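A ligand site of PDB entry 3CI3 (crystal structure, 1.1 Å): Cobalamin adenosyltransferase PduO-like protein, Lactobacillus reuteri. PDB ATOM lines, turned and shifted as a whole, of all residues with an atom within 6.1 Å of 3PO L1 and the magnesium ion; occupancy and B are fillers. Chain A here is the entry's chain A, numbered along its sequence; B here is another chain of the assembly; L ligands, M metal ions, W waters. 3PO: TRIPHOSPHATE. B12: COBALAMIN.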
ATOM      1  N   ILE A   9       0.488  -8.881  -2.156  1.00  0.00           N
ATOM      2  CA  ILE A   9       1.758  -8.171  -2.048  1.00  0.00           C
ATOM      3  C   ILE A   9       2.307  -7.814  -3.412  1.00  0.00           C
ATOM      4  O   ILE A   9       3.175  -6.958  -3.466  1.00  0.00           O
ATOM      5  CB  ILE A   9       2.783  -9.005  -1.237  1.00  0.00           C
ATOM      6  CG1 ILE A   9       3.045 -10.373  -1.871  1.00  0.00           C
ATOM      7  CG2 ILE A   9       2.312  -9.149   0.211  1.00  0.00           C
ATOM      8  CD1 ILE A   9       4.162 -11.195  -1.198  1.00  0.00           C
ATOM      9  N   TYR A  10       1.823  -8.470  -4.474  1.00  0.00           N
ATOM     10  CA  TYR A  10       2.197  -8.124  -5.828  1.00  0.00           C
ATOM     11  C   TYR A  10       1.191  -7.084  -6.349  1.00  0.00           C
ATOM     12  O   TYR A  10      -0.006  -7.408  -6.589  1.00  0.00           O
ATOM     13  CB  TYR A  10       2.321  -9.344  -6.714  1.00  0.00           C
ATOM     14  CG  TYR A  10       1.102 -10.250  -6.846  1.00  0.00           C
ATOM     15  CD1 TYR A  10       0.253 -10.141  -7.959  1.00  0.00           C
ATOM     16  CD2 TYR A  10       0.862 -11.246  -5.909  1.00  0.00           C
ATOM     17  CE1 TYR A  10      -0.840 -10.996  -8.089  1.00  0.00           C
ATOM     18  CE2 TYR A  10      -0.203 -12.062  -6.012  1.00  0.00           C
ATOM     19  CZ  TYR A  10      -1.062 -11.949  -7.103  1.00  0.00           C
ATOM     20  OH  TYR A  10      -2.140 -12.812  -7.243  1.00  0.00           O
ATOM     21  N   THR A  11       1.627  -5.869  -6.421  1.00  0.00           N
ATOM     22  CA  THR A  11       0.828  -4.800  -7.022  1.00  0.00           C
ATOM     23  C   THR A  11       1.043  -4.716  -8.519  1.00  0.00           C
ATOM     24  O   THR A  11       0.188  -4.135  -9.261  1.00  0.00           O
ATOM     25  CB  THR A  11       1.171  -3.447  -6.412  1.00  0.00           C
ATOM     26  OG1 THR A  11       2.447  -2.996  -6.900  1.00  0.00           O
ATOM     27  CG2 THR A  11       1.150  -3.453  -4.875  1.00  0.00           C
ATOM     28  N   LYS A  12       2.161  -5.239  -9.027  1.00  0.00           N
ATOM     29  CA  LYS A  12       2.642  -5.110 -10.403  1.00  0.00           C
ATOM     30  C   LYS A  12       3.099  -3.722 -10.774  1.00  0.00           C
ATOM     31  O   LYS A  12       3.603  -3.535 -11.878  1.00  0.00           O
ATOM     32  CB  LYS A  12       1.637  -5.617 -11.440  1.00  0.00           C
ATOM     33  CG  LYS A  12       1.008  -6.943 -11.041  1.00  0.00           C
ATOM     34  CD  LYS A  12       0.169  -7.497 -12.211  1.00  0.00           C
ATOM     35  CE  LYS A  12      -0.644  -8.713 -11.808  1.00  0.00           C
ATOM     36  NZ  LYS A  12      -1.322  -9.288 -13.020  1.00  0.00           N
ATOM     37  N   ASN A  13       3.022  -2.792  -9.890  1.00  0.00           N
ATOM     38  CA  ASN A  13       3.495  -1.448 -10.194  1.00  0.00           C
ATOM     39  C   ASN A  13       4.986  -1.359 -10.439  1.00  0.00           C
ATOM     40  O   ASN A  13       5.474  -0.403 -11.078  1.00  0.00           O
ATOM     41  CB  ASN A  13       3.089  -0.458  -9.129  1.00  0.00           C
ATOM     42  CG  ASN A  13       1.578  -0.294  -9.095  1.00  0.00           C
ATOM     43  OD1 ASN A  13       0.922  -0.334 -10.141  1.00  0.00           O
ATOM     44  ND2 ASN A  13       1.045  -0.148  -7.940  1.00  0.00           N
ATOM     45  N   GLY A  14       5.761  -2.370  -9.993  1.00  0.00           N
ATOM     46  CA  GLY A  14       7.202  -2.421 -10.223  1.00  0.00           C
ATOM     47  C   GLY A  14       7.579  -3.085 -11.499  1.00  0.00           C
ATOM     48  O   GLY A  14       8.776  -3.222 -11.777  1.00  0.00           O
ATOM     49  N   ASP A  15       6.607  -3.538 -12.285  1.00  0.00           N
ATOM     50  CA  ASP A  15       6.955  -4.387 -13.409  1.00  0.00           C
ATOM     51  C   ASP A  15       7.707  -3.712 -14.554  1.00  0.00           C
ATOM     52  O   ASP A  15       8.309  -4.407 -15.367  1.00  0.00           O
ATOM     53  CB  ASP A  15       5.698  -5.037 -14.075  1.00  0.00           C
ATOM     54  CG  ASP A  15       5.159  -6.238 -13.323  1.00  0.00           C
ATOM     55  OD1 ASP A  15       5.820  -6.714 -12.317  1.00  0.00           O
ATOM     56  OD2 ASP A  15       4.088  -6.766 -13.669  1.00  0.00           O
ATOM     57  N   GLN A  18      10.388   0.753 -12.021  1.00  0.00           N
ATOM     58  CA  GLN A  18      10.349   1.854 -11.054  1.00  0.00           C
ATOM     59  C   GLN A  18       9.668   1.391  -9.774  1.00  0.00           C
ATOM     60  O   GLN A  18       8.795   0.537  -9.791  1.00  0.00           O
ATOM     61  CB  GLN A  18       9.641   3.087 -11.588  1.00  0.00           C
ATOM     62  CG  GLN A  18      10.494   3.846 -12.637  1.00  0.00           C
ATOM     63  CD  GLN A  18       9.619   5.023 -13.189  1.00  0.00           C
ATOM     64  OE1 GLN A  18       8.493   4.803 -13.564  1.00  0.00           O
ATOM     65  NE2 GLN A  18      10.116   6.251 -13.136  1.00  0.00           N
ATOM     66  N   THR A  19       9.982   2.055  -8.673  1.00  0.00           N
ATOM     67  CA  THR A  19       9.409   1.715  -7.382  1.00  0.00           C
ATOM     68  C   THR A  19       9.242   2.981  -6.566  1.00  0.00           C
ATOM     69  O   THR A  19       9.947   3.967  -6.706  1.00  0.00           O
ATOM     70  CB  THR A  19      10.299   0.664  -6.656  1.00  0.00           C
ATOM     71  OG1 THR A  19       9.549  -0.001  -5.621  1.00  0.00           O
ATOM     72  CG2 THR A  19      11.598   1.231  -6.137  1.00  0.00           C
ATOM     73  N   ARG A  20       8.303   2.932  -5.646  1.00  0.00           N
ATOM     74  CA  ARG A  20       8.048   4.031  -4.721  1.00  0.00           C
ATOM     75  C   ARG A  20       8.960   3.956  -3.523  1.00  0.00           C
ATOM     76  O   ARG A  20       9.250   2.827  -2.967  1.00  0.00           O
ATOM     77  CB  ARG A  20       6.624   3.858  -4.188  1.00  0.00           C
ATOM     78  CG  ARG A  20       5.658   4.664  -4.879  1.00  0.00           C
ATOM     79  CD  ARG A  20       5.938   6.155  -4.604  1.00  0.00           C
ATOM     80  NE  ARG A  20       5.515   6.658  -3.307  1.00  0.00           N
ATOM     81  N   LYS A  29      14.747   1.023 -10.019  1.00  0.00           N
ATOM     82  CA  LYS A  29      15.155   0.046  -8.989  1.00  0.00           C
ATOM     83  C   LYS A  29      16.664   0.026  -8.830  1.00  0.00           C
ATOM     84  O   LYS A  29      17.114  -0.426  -7.737  1.00  0.00           O
ATOM     85  CB  LYS A  29      14.597  -1.332  -9.263  1.00  0.00           C
ATOM     86  CG  LYS A  29      13.051  -1.324  -8.926  1.00  0.00           C
ATOM     87  CD  LYS A  29      12.385  -2.600  -9.384  1.00  0.00           C
ATOM     88  CE  LYS A  29      10.932  -2.672  -8.888  1.00  0.00           C
ATOM     89  NZ  LYS A  29      10.202  -3.823  -9.377  1.00  0.00           N
ATOM     90  N   ARG B 138      15.990  -9.541  -5.573  1.00  0.00           N
ATOM     91  CA  ARG B 138      15.817  -8.082  -5.702  1.00  0.00           C
ATOM     92  C   ARG B 138      17.116  -7.421  -6.127  1.00  0.00           C
ATOM     93  O   ARG B 138      17.071  -6.450  -6.941  1.00  0.00           O
ATOM     94  CB  ARG B 138      15.218  -7.536  -4.406  1.00  0.00           C
ATOM     95  CG  ARG B 138      13.807  -8.035  -4.206  1.00  0.00           C
ATOM     96  CD  ARG B 138      13.267  -7.963  -2.802  1.00  0.00           C
ATOM     97  NE  ARG B 138      12.932  -6.596  -2.406  1.00  0.00           N
ATOM     98  CZ  ARG B 138      11.769  -6.027  -2.761  1.00  0.00           C
ATOM     99  NH1 ARG B 138      10.883  -6.664  -3.507  1.00  0.00           N
ATOM    100  NH2 ARG B 138      11.511  -4.807  -2.291  1.00  0.00           N
ATOM    101  N   GLU B 141      17.328  -8.112  -9.760  1.00  0.00           N
ATOM    102  CA  GLU B 141      16.390  -7.198 -10.429  1.00  0.00           C
ATOM    103  C   GLU B 141      16.991  -5.834 -10.616  1.00  0.00           C
ATOM    104  O   GLU B 141      16.806  -5.226 -11.716  1.00  0.00           O
ATOM    105  CB  GLU B 141      15.087  -7.158  -9.619  1.00  0.00           C
ATOM    106  CG  GLU B 141      14.007  -6.391 -10.328  1.00  0.00           C
ATOM    107  CD  GLU B 141      12.757  -6.195  -9.544  1.00  0.00           C
ATOM    108  OE1 GLU B 141      12.742  -6.355  -8.288  1.00  0.00           O
ATOM    109  OE2 GLU B 141      11.718  -5.851 -10.198  1.00  0.00           O
ATOM    110  N   ASN B 162      10.564  -9.560 -10.935  1.00  0.00           N
ATOM    111  CA  ASN B 162       9.831  -8.788  -9.920  1.00  0.00           C
ATOM    112  C   ASN B 162       8.910  -9.696  -9.127  1.00  0.00           C
ATOM    113  O   ASN B 162       8.945  -9.762  -7.863  1.00  0.00           O
ATOM    114  CB  ASN B 162       9.089  -7.651 -10.623  1.00  0.00           C
ATOM    115  CG  ASN B 162       8.363  -6.785  -9.646  1.00  0.00           C
ATOM    116  OD1 ASN B 162       8.842  -6.635  -8.502  1.00  0.00           O
ATOM    117  ND2 ASN B 162       7.252  -6.149 -10.069  1.00  0.00           N
ATOM    118  N   ARG B 163       8.067 -10.436  -9.833  1.00  0.00           N
ATOM    119  CA  ARG B 163       7.115 -11.316  -9.115  1.00  0.00           C
ATOM    120  C   ARG B 163       7.819 -12.350  -8.236  1.00  0.00           C
ATOM    121  O   ARG B 163       7.292 -12.706  -7.172  1.00  0.00           O
ATOM    122  CB  ARG B 163       6.170 -11.996 -10.121  1.00  0.00           C
ATOM    123  CG  ARG B 163       4.839 -12.409  -9.483  1.00  0.00           C
ATOM    124  CD  ARG B 163       3.888 -11.205  -9.241  1.00  0.00           C
ATOM    125  NE  ARG B 163       3.387 -10.646 -10.516  1.00  0.00           N
ATOM    126  CZ  ARG B 163       3.862  -9.570 -11.143  1.00  0.00           C
ATOM    127  NH1 ARG B 163       4.765  -8.773 -10.627  1.00  0.00           N
ATOM    128  NH2 ARG B 163       3.387  -9.301 -12.370  1.00  0.00           N
ATOM    129  N   SER B 165      10.407 -12.203  -6.350  1.00  0.00           N
ATOM    130  CA  SER B 165      10.751 -11.851  -4.944  1.00  0.00           C
ATOM    131  C   SER B 165       9.533 -11.812  -4.023  1.00  0.00           C
ATOM    132  O   SER B 165       9.673 -12.099  -2.821  1.00  0.00           O
ATOM    133  CB  SER B 165      11.603 -10.617  -4.804  1.00  0.00           C
ATOM    134  OG  SER B 165      10.904  -9.430  -5.133  1.00  0.00           O
ATOM    135  N   ASP B 166       8.365 -11.476  -4.579  1.00  0.00           N
ATOM    136  CA  ASP B 166       7.132 -11.654  -3.784  1.00  0.00           C
ATOM    137  C   ASP B 166       6.877 -13.134  -3.531  1.00  0.00           C
ATOM    138  O   ASP B 166       6.454 -13.492  -2.388  1.00  0.00           O
ATOM    139  CB  ASP B 166       5.958 -10.986  -4.501  1.00  0.00           C
ATOM    140  CG  ASP B 166       5.951  -9.508  -4.431  1.00  0.00           C
ATOM    141  OD1 ASP B 166       6.701  -8.826  -3.710  1.00  0.00           O
ATOM    142  OD2 ASP B 166       5.143  -8.909  -5.242  1.00  0.00           O
HETATM  143  PG  3PO L   1       7.944  -4.262  -3.885  1.00  0.00           P
HETATM  144  O1G 3PO L   1       6.560  -4.512  -3.381  1.00  0.00           O
HETATM  145  O2G 3PO L   1       8.912  -3.802  -2.820  1.00  0.00           O
HETATM  146  O3G 3PO L   1       8.573  -5.387  -4.639  1.00  0.00           O
HETATM  147  PB  3PO L   1       7.588  -2.929  -6.468  1.00  0.00           P
HETATM  148  O1B 3PO L   1       8.458  -3.932  -7.174  1.00  0.00           O
HETATM  149  O2B 3PO L   1       7.678  -1.489  -6.896  1.00  0.00           O
HETATM  150  O3B 3PO L   1       7.832  -3.030  -4.928  1.00  0.00           O
HETATM  151  PA  3PO L   1       5.459  -4.836  -7.095  1.00  0.00           P
HETATM  152  O1A 3PO L   1       6.496  -5.867  -6.681  1.00  0.00           O
HETATM  153  O2A 3PO L   1       4.201  -4.947  -6.280  1.00  0.00           O
HETATM  154  O3A 3PO L   1       6.037  -3.381  -6.614  1.00  0.00           O
HETATM  155  O5' 3PO L   1       5.264  -4.670  -8.580  1.00  0.00           O
HETATM  156 CO   B12 L   2       8.125  -2.748   1.195  1.00  0.00          CO
HETATM  157  N21 B12 L   2       6.318  -2.833   0.549  1.00  0.00           N
HETATM  158  N22 B12 L   2       8.212  -4.634   1.120  1.00  0.00           N
HETATM  159  N23 B12 L   2       9.852  -2.480   2.001  1.00  0.00           N
HETATM  160  N24 B12 L   2       7.743  -1.006   1.284  1.00  0.00           N
HETATM  161  C1  B12 L   2       5.583  -1.581   0.559  1.00  0.00           C
HETATM  162  C20 B12 L   2       4.917  -1.577   1.957  1.00  0.00           C
HETATM  163  C2  B12 L   2       4.549  -1.748  -0.577  1.00  0.00           C
HETATM  164  C25 B12 L   2       3.193  -0.999  -0.323  1.00  0.00           C
HETATM  165  C26 B12 L   2       5.179  -1.358  -1.889  1.00  0.00           C
HETATM  166  C27 B12 L   2       4.333  -1.631  -3.151  1.00  0.00           C
HETATM  167  O28 B12 L   2       4.566  -2.589  -3.890  1.00  0.00           O
HETATM  168  N29 B12 L   2       3.290  -0.812  -3.393  1.00  0.00           N
HETATM  169  C3  B12 L   2       4.395  -3.291  -0.608  1.00  0.00           C
HETATM  170  C30 B12 L   2       3.138  -3.884   0.110  1.00  0.00           C
HETATM  171  C31 B12 L   2       1.961  -3.984  -0.895  1.00  0.00           C
HETATM  172  C32 B12 L   2       0.626  -4.270  -0.198  1.00  0.00           C
HETATM  173  O34 B12 L   2       0.340  -3.671   0.846  1.00  0.00           O
HETATM  174  N33 B12 L   2      -0.271  -5.104  -0.731  1.00  0.00           N
HETATM  175  C4  B12 L   2       5.693  -3.794  -0.064  1.00  0.00           C
HETATM  176  C5  B12 L   2       6.175  -5.135  -0.111  1.00  0.00           C
HETATM  177  C35 B12 L   2       5.275  -6.120  -0.816  1.00  0.00           C
HETATM  178  C6  B12 L   2       7.340  -5.541   0.467  1.00  0.00           C
HETATM  179  C7  B12 L   2       7.987  -6.921   0.443  1.00  0.00           C
HETATM  180  C36 B12 L   2       7.046  -8.101   0.611  1.00  0.00           C
HETATM  181  C37 B12 L   2       8.689  -6.986  -0.944  1.00  0.00           C
HETATM  182  C38 B12 L   2       9.460  -8.256  -1.171  1.00  0.00           C
HETATM  183  O39 B12 L   2      10.582  -8.466  -0.621  1.00  0.00           O
HETATM  184  N40 B12 L   2       8.932  -9.189  -1.933  1.00  0.00           N
HETATM  185  C8  B12 L   2       8.998  -6.843   1.587  1.00  0.00           C
HETATM  186  C41 B12 L   2       8.486  -7.260   2.962  1.00  0.00           C
HETATM  187  C42 B12 L   2       9.599  -7.172   4.004  1.00  0.00           C
HETATM  188  C43 B12 L   2       9.269  -7.763   5.351  1.00  0.00           C
HETATM  189  O44 B12 L   2       8.151  -7.767   5.802  1.00  0.00           O
HETATM  190  N45 B12 L   2      10.312  -8.341   5.986  1.00  0.00           N
HETATM  191  C9  B12 L   2       9.268  -5.381   1.563  1.00  0.00           C
HETATM  192  C10 B12 L   2      10.474  -4.808   1.993  1.00  0.00           C
HETATM  193  C11 B12 L   2      10.708  -3.529   2.214  1.00  0.00           C
HETATM  194  C12 B12 L   2      12.033  -2.930   2.678  1.00  0.00           C
HETATM  195  C46 B12 L   2      12.706  -3.827   3.753  1.00  0.00           C
HETATM  196  C47 B12 L   2      12.976  -2.871   1.485  1.00  0.00           C
HETATM  197  C13 B12 L   2      11.641  -1.523   3.137  1.00  0.00           C
HETATM  198  C48 B12 L   2      11.331  -1.402   4.621  1.00  0.00           C
HETATM  199  C49 B12 L   2      12.536  -1.105   5.544  1.00  0.00           C
HETATM  200  C50 B12 L   2      13.414  -0.091   4.916  1.00  0.00           C
HETATM  201  O51 B12 L   2      14.530  -0.406   4.497  1.00  0.00           O
HETATM  202  N52 B12 L   2      12.902   1.131   4.906  1.00  0.00           N
HETATM  203  C14 B12 L   2      10.339  -1.317   2.496  1.00  0.00           C
HETATM  204  C15 B12 L   2       9.738  -0.018   2.252  1.00  0.00           C
HETATM  205  C53 B12 L   2      10.546   1.177   2.718  1.00  0.00           C
HETATM  206  C16 B12 L   2       8.524   0.061   1.663  1.00  0.00           C
HETATM  207  C17 B12 L   2       7.766   1.401   1.491  1.00  0.00           C
HETATM  208  C54 B12 L   2       8.493   2.200   0.395  1.00  0.00           C
HETATM  209  C55 B12 L   2       7.590   2.269   2.780  1.00  0.00           C
HETATM  210  C56 B12 L   2       7.327   1.420   4.017  1.00  0.00           C
HETATM  211  C57 B12 L   2       6.989   2.204   5.283  1.00  0.00           C
HETATM  212  O58 B12 L   2       7.809   2.241   6.189  1.00  0.00           O
HETATM  213  N59 B12 L   2       5.815   2.833   5.247  1.00  0.00           N
HETATM  214  C18 B12 L   2       6.428   0.944   0.908  1.00  0.00           C
HETATM  215  C60 B12 L   2       5.904   1.851  -0.255  1.00  0.00           C
HETATM  216  C61 B12 L   2       5.513   3.253   0.249  1.00  0.00           C
HETATM  217  O63 B12 L   2       4.710   3.401   1.191  1.00  0.00           O
HETATM  218  N62 B12 L   2       6.064   4.311  -0.367  1.00  0.00           N
HETATM  219  C19 B12 L   2       6.587  -0.508   0.591  1.00  0.00           C
HETATM  220  C1P B12 L   2       5.258   3.517   6.433  1.00  0.00           C
HETATM  221  C2P B12 L   2       5.223   5.004   6.203  1.00  0.00           C
HETATM  222  C3P B12 L   2       6.636   5.530   6.312  1.00  0.00           C
HETATM  223  O3  B12 L   2       4.767   5.237   4.873  1.00  0.00           O
HETATM  224  O4  B12 L   2       3.625   7.467   5.353  1.00  0.00           O
HETATM  225  O5  B12 L   2       3.191   6.307   3.145  1.00  0.00           O
HETATM  226  P   B12 L   2       3.458   6.144   4.635  1.00  0.00           P
HETATM  227  O2  B12 L   2       2.245   5.319   5.310  1.00  0.00           O
HETATM  228 MG    MG M   1       8.544  -5.929  -6.602  1.00  0.00          MG
HETATM  229  O   HOH W   1       8.533  -7.875  -5.980  1.00  0.00           O
HETATM  230  O   HOH W   2      10.776  -1.927  -4.114  1.00  0.00           O
HETATM  231  O   HOH W   3       5.565  -8.388  -7.877  1.00  0.00           O
HETATM  232  O   HOH W   4      10.641  -5.756  -6.631  1.00  0.00           O
HETATM  233  O   HOH W   5       9.251  -2.050  -1.098  1.00  0.00           O
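The backbone NH (N) of Thr 11 lies within hydrogen-bond range of an oxygen (O2A) of 3PO L1 (2.7 Å).
O2A of 3PO L1 lies within hydrogen-bond range of OG1 of Thr 11, 2.7 Å away.
O2B of 3PO L1 is in hydrogen-bond range of OG1 of Thr 19 (2.7 Å).
The backbone NH (N) of Gly 14 is in hydrogen-bond range of an oxygen (O5') of 3PO L1, at 2.7 Å.
NZ of Lys 29 lies close to O1B of 3PO L1 (2.8 Å).
O2G of 3PO L1 lies within salt-bridge range of NH2 of Arg 138 of chain B, 2.8 Å away.
An oxygen (O5') of 3PO L1 is in hydrogen-bond range of the backbone NH of Lys 12, 3.2 Å away.
N of Asn 13 lies within hydrogen-bond range of O5' of 3PO L1 (3.2 Å).
The guanidinium group (NH1) of Arg 138 of chain B sits close to an oxygen (O39) of B12 L2 (3.4 Å).
A nitrogen (N40) of B12 L2 sits at hydrogen-bond distance from the side-chain carboxylate (OD1) of Asp 166 of chain B, 2.9 Å away.
The backbone carbonyl oxygen of Ser 165 of chain B sits at hydrogen-bond distance from a nitrogen (N40) of B12 L2, at 3.1 Å.
The side-chain amide oxygen of Asn 162 of chain B lies close to the side-chain amino group of Lys 29 (3.2 Å).
The side-chain carboxylate of Asp 15 lies within hydrogen-bond range of the side-chain amide nitrogen of Asn 162 of chain B, at 2.7 Å.
OG of Ser 165 of chain B lies within hydrogen-bond range of O of Asn 162 of chain B (3.4 Å).
The side-chain amide oxygen (OD1) of Asn 162 of chain B sits close to the side-chain carboxylate (OE2) of Glu 141 of chain B, 3.4 Å away.
The side-chain hydroxyl (OG1) of Thr 11 sits at hydrogen-bond distance from the backbone NH (N) of Asn 13 (3.1 Å).
The side-chain amino group (NZ) of Lys 29 sits at hydrogen-bond distance from the backbone carbonyl oxygen (O) of Gly 14, at 2.9 Å.
The side-chain amino group of Lys 29 is in salt-bridge range of the side-chain carboxylate of Glu 141 of chain B, 2.7 Å away.
OG of Ser 165 of chain B lies within hydrogen-bond range of NH1 of Arg 138 of chain B, at 3.2 Å.
Water W4 lies within hydrogen-bond range of OE1 of Glu 141 of chain B, NH1 of Arg 138 of chain B and NZ of Lys 29.
Water W1 lies within hydrogen-bond range of the backbone carbonyl oxygen of Asn 162 of chain B (2.7 Å), the side-chain hydroxyl of Ser 165 of chain B (3.0 Å) and the side-chain carboxylate of Asp 166 of chain B (3.1 Å).
Water W3 lies within hydrogen-bond range of the side-chain carboxylate (OD2) of Asp 166 of chain B (2.7 Å) and the guanidinium group (NH1) of Arg 163 of chain B (2.9 Å).
Water W2 lies within hydrogen-bond range of the side-chain hydroxyl of Thr 19 (2.7 Å), an oxygen (O2G) of 3PO L1 (2.9 Å) and the guanidinium group of Arg 138 of chain B (3.5 Å).
Residues that only touch the magnesium ion: Lys 29 and Arg 138 of chain B.
Of the 17 residues printed, 3 come within 4 Å of the magnesium ion.
The nearest printed residue that does not touch the magnesium ion is Ser 165 of chain B (4.5 Å).
Merely in contact with 3PO L1: Ile 9 (3.6 Å), Tyr 10 (3.7 Å), Gln 18 (3.7 Å) and Asp 166 of chain B (3.6 Å).
Within 4 Å of 3PO L1: Ile 9, Tyr 10, Thr 11, Lys 12, Asn 13, Gly 14, Gln 18, Thr 19, Lys 29, Arg 138 of chain B, Asn 162 of chain B and Asp 166 of chain B.
An oxygen (O1G) of 3PO L1 lies close to an oxygen (O28) of B12 L2 (2.8 Å).
The magnesium ion is bound by an oxygen (O3G) of 3PO L1 (2.0 Å), water W1 (2.0 Å), the side-chain amide oxygen (OD1) of Asn 162 of chain B (2.0 Å), an oxygen (O1A) of 3PO L1 (2.1 Å), an oxygen (O1B) of 3PO L1 (2.1 Å) and water W4 (2.1 Å).
The magnesium ion has six donor atoms within binding distance.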
